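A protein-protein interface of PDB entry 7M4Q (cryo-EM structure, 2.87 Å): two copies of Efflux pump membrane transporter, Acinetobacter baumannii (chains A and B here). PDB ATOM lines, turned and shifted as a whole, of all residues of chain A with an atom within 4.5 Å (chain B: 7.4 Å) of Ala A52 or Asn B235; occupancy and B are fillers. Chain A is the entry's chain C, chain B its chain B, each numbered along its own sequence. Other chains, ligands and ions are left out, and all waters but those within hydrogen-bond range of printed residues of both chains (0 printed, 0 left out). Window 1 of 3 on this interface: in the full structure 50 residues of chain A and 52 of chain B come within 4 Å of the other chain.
The side-chain amide oxygen of Gln A729 lies close to the side-chain amide oxygen of Gln B237, at 3.3 Å. The backbone carbonyl oxygen (O) of Asn B235 is in hydrogen-bond range of the backbone NH (N) of Ile A730, at 2.8 Å. The backbone carbonyl oxygen of Gly A84 lies within hydrogen-bond range of the side-chain amide nitrogen of Asn B235 (3.5 Å). N of Tyr A728 is in hydrogen-bond range of O of Thr B233, at 3.1 Å. The backbone carbonyl oxygen (O) of Tyr A728 lies within hydrogen-bond range of the backbone NH (N) of Asn B235 (3.1 Å). O of Gly A51 lies close to OE1 of Gln B213 (3.5 Å). The side-chain amide oxygen (OE1) of Gln A729 lies close to the backbone carbonyl oxygen (O) of Asn B235 (3.3 Å). N of Gln B237 sits at hydrogen-bond distance from O of Ile A730 (2.9 Å).
The backbone NH of Val B234 sits at hydrogen-bond distance from the backbone carbonyl oxygen of Gly B217. OE1 of Gln B213 lies close to O of Ala B236. The side-chain hydroxyl of Ser A53 sits at hydrogen-bond distance from the side-chain hydroxyl of Thr A56, at 2.8 Å.
No position is printed for both chains. Of the 17 pairs that touch across the chains among the printed residues, none has its exchanged pair printed and touching as well.
Hydrophobic or aromatic side chains of chain B that line the printed part of chain A: Val B234 and Ala B236. Of the 13 printed residues of chain A, 8 touch a printed residue of chain B. Among the printed residues, no Asp or Glu carboxylate lies within 4 Å of a Lys or Arg side-chain nitrogen of the other chain.
Pro A50 touches Gln B213 (O to CG, 3.8 Å). Val B214 touches Gly A51. Gly A51 touches Asn B235 (O to OD1, 3.8 Å). Ala A52 touches Asn B235. Ser A53 touches Asn B235. Val B234 touches Tyr A728 (CA to O, 3.4 Å). C of Ala B236 touches OE1 of Gln A729 (3.8 Å). Val B234 touches Ile A730 (CG1 to CG1, 3.8 Å). O of Ile A730 touches CA of Ala B236, 3.2 Å away.
Ala A52 touches just one residue of chain B: Asn B235. Of chain A, only Gly A51 (3.8 Å), Ala A52 (3.95 Å), Ser A53 (3.6 Å), Gly A84 (3.5 Å), Tyr A728 (3.1 Å), Gln A729 (3.3 Å) and Ile A730 (2.8 Å) come within 4 Å of Asn B235. Gly A51 touches three residues of chain B. Of the printed residues of chain A, Gln B213 touches Pro A50 (3.8 Å) and Gly A51 (3.5 Å). Printed residues of chain A within 4 Å of Gln B237: Gln A729 and Ile A730. Printed residues of chain B within 4 Å of Pro A50: Gln B213 (3.8 Å). Printed residues of chain B within 4 Å of Gly A84: Asn B235 (3.5 Å). Of the printed residues of chain B, Tyr A728 touches Thr B233, Val B234 and Asn B235. Ala B232 touches none of the printed residues of chain A. The nearest residue of chain B that does not touch Ala A52 is Gln B213 (4.7 Å). The nearest printed residue of chain A that does not touch Asn B235 is Ala A54 (5.0 Å). The nearest printed residue of chain B that does not touch Tyr A728 is Ala B232 (5.0 Å).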
ATOM      1  N   TYR A  49       1.874   4.807  28.891  1.00  0.00           N
ATOM      2  CA  TYR A  49       1.634   6.223  28.621  1.00  0.00           C
ATOM      3  C   TYR A  49       0.361   6.292  27.788  1.00  0.00           C
ATOM      4  O   TYR A  49       0.416   6.306  26.553  1.00  0.00           O
ATOM      5  CB  TYR A  49       2.822   6.854  27.896  1.00  0.00           C
ATOM      6  CG  TYR A  49       2.810   8.361  27.759  1.00  0.00           C
ATOM      7  CD1 TYR A  49       1.664   9.094  27.952  1.00  0.00           C
ATOM      8  CD2 TYR A  49       3.963   9.042  27.415  1.00  0.00           C
ATOM      9  CE1 TYR A  49       1.660  10.451  27.821  1.00  0.00           C
ATOM     10  CE2 TYR A  49       3.972  10.417  27.285  1.00  0.00           C
ATOM     11  CZ  TYR A  49       2.811  11.114  27.485  1.00  0.00           C
ATOM     12  OH  TYR A  49       2.785  12.477  27.360  1.00  0.00           O
ATOM     13  N   PRO A  50      -0.807   6.313  28.427  1.00  0.00           N
ATOM     14  CA  PRO A  50      -2.059   6.294  27.658  1.00  0.00           C
ATOM     15  C   PRO A  50      -2.152   7.455  26.681  1.00  0.00           C
ATOM     16  O   PRO A  50      -2.003   8.618  27.053  1.00  0.00           O
ATOM     17  CB  PRO A  50      -3.139   6.372  28.742  1.00  0.00           C
ATOM     18  CG  PRO A  50      -2.445   6.805  29.973  1.00  0.00           C
ATOM     19  CD  PRO A  50      -1.056   6.334  29.877  1.00  0.00           C
ATOM     20  N   GLY A  51      -2.419   7.126  25.421  1.00  0.00           N
ATOM     21  CA  GLY A  51      -2.611   8.095  24.375  1.00  0.00           C
ATOM     22  C   GLY A  51      -1.420   8.298  23.467  1.00  0.00           C
ATOM     23  O   GLY A  51      -1.586   8.827  22.366  1.00  0.00           O
ATOM     24  N   ALA A  52      -0.232   7.886  23.892  1.00  0.00           N
ATOM     25  CA  ALA A  52       0.983   8.191  23.161  1.00  0.00           C
ATOM     26  C   ALA A  52       1.259   7.167  22.070  1.00  0.00           C
ATOM     27  O   ALA A  52       0.874   6.003  22.167  1.00  0.00           O
ATOM     28  CB  ALA A  52       2.167   8.265  24.119  1.00  0.00           C
ATOM     29  N   SER A  53       1.961   7.616  21.036  1.00  0.00           N
ATOM     30  CA  SER A  53       2.417   6.766  19.951  1.00  0.00           C
ATOM     31  C   SER A  53       3.658   5.988  20.364  1.00  0.00           C
ATOM     32  O   SER A  53       4.360   6.342  21.311  1.00  0.00           O
ATOM     33  CB  SER A  53       2.744   7.602  18.729  1.00  0.00           C
ATOM     34  OG  SER A  53       3.837   8.458  19.003  1.00  0.00           O
ATOM     35  N   ALA A  54       3.947   4.933  19.603  1.00  0.00           N
ATOM     36  CA  ALA A  54       5.105   4.096  19.889  1.00  0.00           C
ATOM     37  C   ALA A  54       6.384   4.914  19.933  1.00  0.00           C
ATOM     38  O   ALA A  54       7.270   4.656  20.756  1.00  0.00           O
ATOM     39  CB  ALA A  54       5.221   2.996  18.837  1.00  0.00           C
ATOM     40  N   THR A  56       6.730   8.201  20.643  1.00  0.00           N
ATOM     41  CA  THR A  56       6.790   8.995  21.858  1.00  0.00           C
ATOM     42  C   THR A  56       7.137   8.121  23.050  1.00  0.00           C
ATOM     43  O   THR A  56       7.902   8.533  23.924  1.00  0.00           O
ATOM     44  CB  THR A  56       5.469   9.726  22.088  1.00  0.00           C
ATOM     45  OG1 THR A  56       4.996  10.275  20.855  1.00  0.00           O
ATOM     46  CG2 THR A  56       5.658  10.855  23.060  1.00  0.00           C
ATOM     47  N   VAL A  57       6.580   6.908  23.106  1.00  0.00           N
ATOM     48  CA  VAL A  57       6.889   5.995  24.202  1.00  0.00           C
ATOM     49  C   VAL A  57       8.371   5.681  24.215  1.00  0.00           C
ATOM     50  O   VAL A  57       9.033   5.761  25.253  1.00  0.00           O
ATOM     51  CB  VAL A  57       6.056   4.705  24.087  1.00  0.00           C
ATOM     52  CG1 VAL A  57       6.497   3.700  25.127  1.00  0.00           C
ATOM     53  CG2 VAL A  57       4.582   5.002  24.217  1.00  0.00           C
ATOM     54  N   GLY A  84       2.188   0.945  20.157  1.00  0.00           N
ATOM     55  CA  GLY A  84       1.336   2.059  19.790  1.00  0.00           C
ATOM     56  C   GLY A  84       0.173   2.268  20.724  1.00  0.00           C
ATOM     57  O   GLY A  84      -0.453   3.326  20.691  1.00  0.00           O
ATOM     58  N   GLY A  86       0.627   2.561  23.834  1.00  0.00           N
ATOM     59  CA  GLY A  86       1.161   3.277  24.965  1.00  0.00           C
ATOM     60  C   GLY A  86       1.915   2.447  25.970  1.00  0.00           C
ATOM     61  O   GLY A  86       2.102   2.903  27.099  1.00  0.00           O
ATOM     62  N   TYR A 728      -5.206   4.889  12.230  1.00  0.00           N
ATOM     63  CA  TYR A 728      -6.018   6.084  12.071  1.00  0.00           C
ATOM     64  C   TYR A 728      -5.496   7.171  12.999  1.00  0.00           C
ATOM     65  O   TYR A 728      -5.276   6.925  14.186  1.00  0.00           O
ATOM     66  CB  TYR A 728      -7.488   5.782  12.352  1.00  0.00           C
ATOM     67  CG  TYR A 728      -8.418   6.796  11.753  1.00  0.00           C
ATOM     68  CD1 TYR A 728      -8.699   6.787  10.405  1.00  0.00           C
ATOM     69  CD2 TYR A 728      -9.013   7.767  12.538  1.00  0.00           C
ATOM     70  CE1 TYR A 728      -9.535   7.716   9.854  1.00  0.00           C
ATOM     71  CE2 TYR A 728      -9.852   8.696  11.995  1.00  0.00           C
ATOM     72  CZ  TYR A 728     -10.108   8.664  10.646  1.00  0.00           C
ATOM     73  OH  TYR A 728     -10.946   9.582  10.086  1.00  0.00           O
ATOM     74  N   GLN A 729      -5.287   8.363  12.455  1.00  0.00           N
ATOM     75  CA  GLN A 729      -4.685   9.473  13.176  1.00  0.00           C
ATOM     76  C   GLN A 729      -5.702  10.592  13.317  1.00  0.00           C
ATOM     77  O   GLN A 729      -6.310  11.003  12.329  1.00  0.00           O
ATOM     78  CB  GLN A 729      -3.439   9.980  12.449  1.00  0.00           C
ATOM     79  CG  GLN A 729      -2.730  11.124  13.139  1.00  0.00           C
ATOM     80  CD  GLN A 729      -2.223  10.768  14.522  1.00  0.00           C
ATOM     81  OE1 GLN A 729      -2.344  11.552  15.454  1.00  0.00           O
ATOM     82  NE2 GLN A 729      -1.637   9.589  14.656  1.00  0.00           N
ATOM     83  N   ILE A 730      -5.854  11.086  14.535  1.00  0.00           N
ATOM     84  CA  ILE A 730      -6.785  12.154  14.801  1.00  0.00           C
ATOM     85  C   ILE A 730      -6.065  13.416  15.164  1.00  0.00           C
ATOM     86  O   ILE A 730      -5.292  13.439  16.101  1.00  0.00           O
ATOM     87  CB  ILE A 730      -7.713  11.814  15.958  1.00  0.00           C
ATOM     88  CG1 ILE A 730      -8.518  10.579  15.617  1.00  0.00           C
ATOM     89  CG2 ILE A 730      -8.625  12.985  16.256  1.00  0.00           C
ATOM     90  CD1 ILE A 730      -9.994  10.792  15.736  1.00  0.00           C
ATOM     91  N   GLN B 213      -3.413  15.316  26.681  1.00  0.00           N
ATOM     92  CA  GLN B 213      -3.267  14.175  25.794  1.00  0.00           C
ATOM     93  C   GLN B 213      -4.577  13.396  25.771  1.00  0.00           C
ATOM     94  O   GLN B 213      -5.099  13.031  26.823  1.00  0.00           O
ATOM     95  CB  GLN B 213      -2.115  13.287  26.258  1.00  0.00           C
ATOM     96  CG  GLN B 213      -1.907  12.066  25.420  1.00  0.00           C
ATOM     97  CD  GLN B 213      -1.641  12.409  23.983  1.00  0.00           C
ATOM     98  OE1 GLN B 213      -2.439  12.111  23.099  1.00  0.00           O
ATOM     99  NE2 GLN B 213      -0.519  13.053  23.739  1.00  0.00           N
ATOM    100  N   VAL B 214      -5.098  13.141  24.573  1.00  0.00           N
ATOM    101  CA  VAL B 214      -6.377  12.465  24.366  1.00  0.00           C
ATOM    102  C   VAL B 214      -6.128  11.009  24.001  1.00  0.00           C
ATOM    103  O   VAL B 214      -5.174  10.693  23.284  1.00  0.00           O
ATOM    104  CB  VAL B 214      -7.185  13.175  23.260  1.00  0.00           C
ATOM    105  CG1 VAL B 214      -8.396  12.363  22.868  1.00  0.00           C
ATOM    106  CG2 VAL B 214      -7.593  14.556  23.697  1.00  0.00           C
ATOM    107  N   ALA B 215      -6.992  10.121  24.488  1.00  0.00           N
ATOM    108  CA  ALA B 215      -6.975   8.702  24.157  1.00  0.00           C
ATOM    109  C   ALA B 215      -8.274   8.333  23.446  1.00  0.00           C
ATOM    110  O   ALA B 215      -9.333   8.865  23.774  1.00  0.00           O
ATOM    111  CB  ALA B 215      -6.802   7.865  25.418  1.00  0.00           C
ATOM    112  N   VAL B 216      -8.191   7.460  22.436  1.00  0.00           N
ATOM    113  CA  VAL B 216      -9.376   7.135  21.641  1.00  0.00           C
ATOM    114  C   VAL B 216      -9.558   5.647  21.351  1.00  0.00           C
ATOM    115  O   VAL B 216     -10.334   5.286  20.461  1.00  0.00           O
ATOM    116  CB  VAL B 216      -9.368   7.906  20.307  1.00  0.00           C
ATOM    117  CG1 VAL B 216     -10.772   7.984  19.742  1.00  0.00           C
ATOM    118  CG2 VAL B 216      -8.784   9.285  20.468  1.00  0.00           C
ATOM    119  N   GLY B 217      -8.858   4.771  22.059  1.00  0.00           N
ATOM    120  CA  GLY B 217      -9.122   3.339  21.905  1.00  0.00           C
ATOM    121  C   GLY B 217      -8.767   2.756  20.544  1.00  0.00           C
ATOM    122  O   GLY B 217      -7.724   3.053  19.961  1.00  0.00           O
ATOM    123  N   ALA B 232      -8.004  -1.553  14.118  1.00  0.00           N
ATOM    124  CA  ALA B 232      -6.891  -0.625  14.002  1.00  0.00           C
ATOM    125  C   ALA B 232      -6.793   0.259  15.236  1.00  0.00           C
ATOM    126  O   ALA B 232      -7.782   0.505  15.924  1.00  0.00           O
ATOM    127  CB  ALA B 232      -7.031   0.232  12.747  1.00  0.00           C
ATOM    128  N   THR B 233      -5.579   0.726  15.506  1.00  0.00           N
ATOM    129  CA  THR B 233      -5.327   1.688  16.569  1.00  0.00           C
ATOM    130  C   THR B 233      -5.723   3.095  16.137  1.00  0.00           C
ATOM    131  O   THR B 233      -5.559   3.465  14.974  1.00  0.00           O
ATOM    132  CB  THR B 233      -3.849   1.672  16.951  1.00  0.00           C
ATOM    133  OG1 THR B 233      -3.510   0.387  17.471  1.00  0.00           O
ATOM    134  CG2 THR B 233      -3.558   2.702  18.002  1.00  0.00           C
ATOM    135  N   VAL B 234      -6.237   3.880  17.084  1.00  0.00           N
ATOM    136  CA  VAL B 234      -6.622   5.270  16.843  1.00  0.00           C
ATOM    137  C   VAL B 234      -5.857   6.158  17.807  1.00  0.00           C
ATOM    138  O   VAL B 234      -6.199   6.233  18.992  1.00  0.00           O
ATOM    139  CB  VAL B 234      -8.129   5.500  17.007  1.00  0.00           C
ATOM    140  CG1 VAL B 234      -8.479   6.904  16.543  1.00  0.00           C
ATOM    141  CG2 VAL B 234      -8.923   4.459  16.254  1.00  0.00           C
ATOM    142  N   ASN B 235      -4.868   6.880  17.295  1.00  0.00           N
ATOM    143  CA  ASN B 235      -4.091   7.818  18.087  1.00  0.00           C
ATOM    144  C   ASN B 235      -4.457   9.249  17.720  1.00  0.00           C
ATOM    145  O   ASN B 235      -4.728   9.553  16.558  1.00  0.00           O
ATOM    146  CB  ASN B 235      -2.591   7.589  17.894  1.00  0.00           C
ATOM    147  CG  ASN B 235      -2.024   6.573  18.875  1.00  0.00           C
ATOM    148  OD1 ASN B 235      -2.650   6.233  19.870  1.00  0.00           O
ATOM    149  ND2 ASN B 235      -0.820   6.098  18.598  1.00  0.00           N
ATOM    150  N   ALA B 236      -4.462  10.118  18.728  1.00  0.00           N
ATOM    151  CA  ALA B 236      -4.765  11.534  18.585  1.00  0.00           C
ATOM    152  C   ALA B 236      -3.545  12.365  18.955  1.00  0.00           C
ATOM    153  O   ALA B 236      -2.782  11.998  19.850  1.00  0.00           O
ATOM    154  CB  ALA B 236      -5.945  11.933  19.466  1.00  0.00           C
ATOM    155  N   GLN B 237      -3.366  13.505  18.286  1.00  0.00           N
ATOM    156  CA  GLN B 237      -2.287  14.425  18.581  1.00  0.00           C
ATOM    157  C   GLN B 237      -2.993  15.665  19.118  1.00  0.00           C
ATOM    158  O   GLN B 237      -3.742  16.293  18.398  1.00  0.00           O
ATOM    159  CB  GLN B 237      -1.511  14.788  17.341  1.00  0.00           C
ATOM    160  CG  GLN B 237      -0.014  14.840  17.558  1.00  0.00           C
ATOM    161  CD  GLN B 237       0.582  13.495  17.943  1.00  0.00           C
ATOM    162  OE1 GLN B 237       0.057  12.433  17.595  1.00  0.00           O
ATOM    163  NE2 GLN B 237       1.696  13.537  18.654  1.00  0.00           N
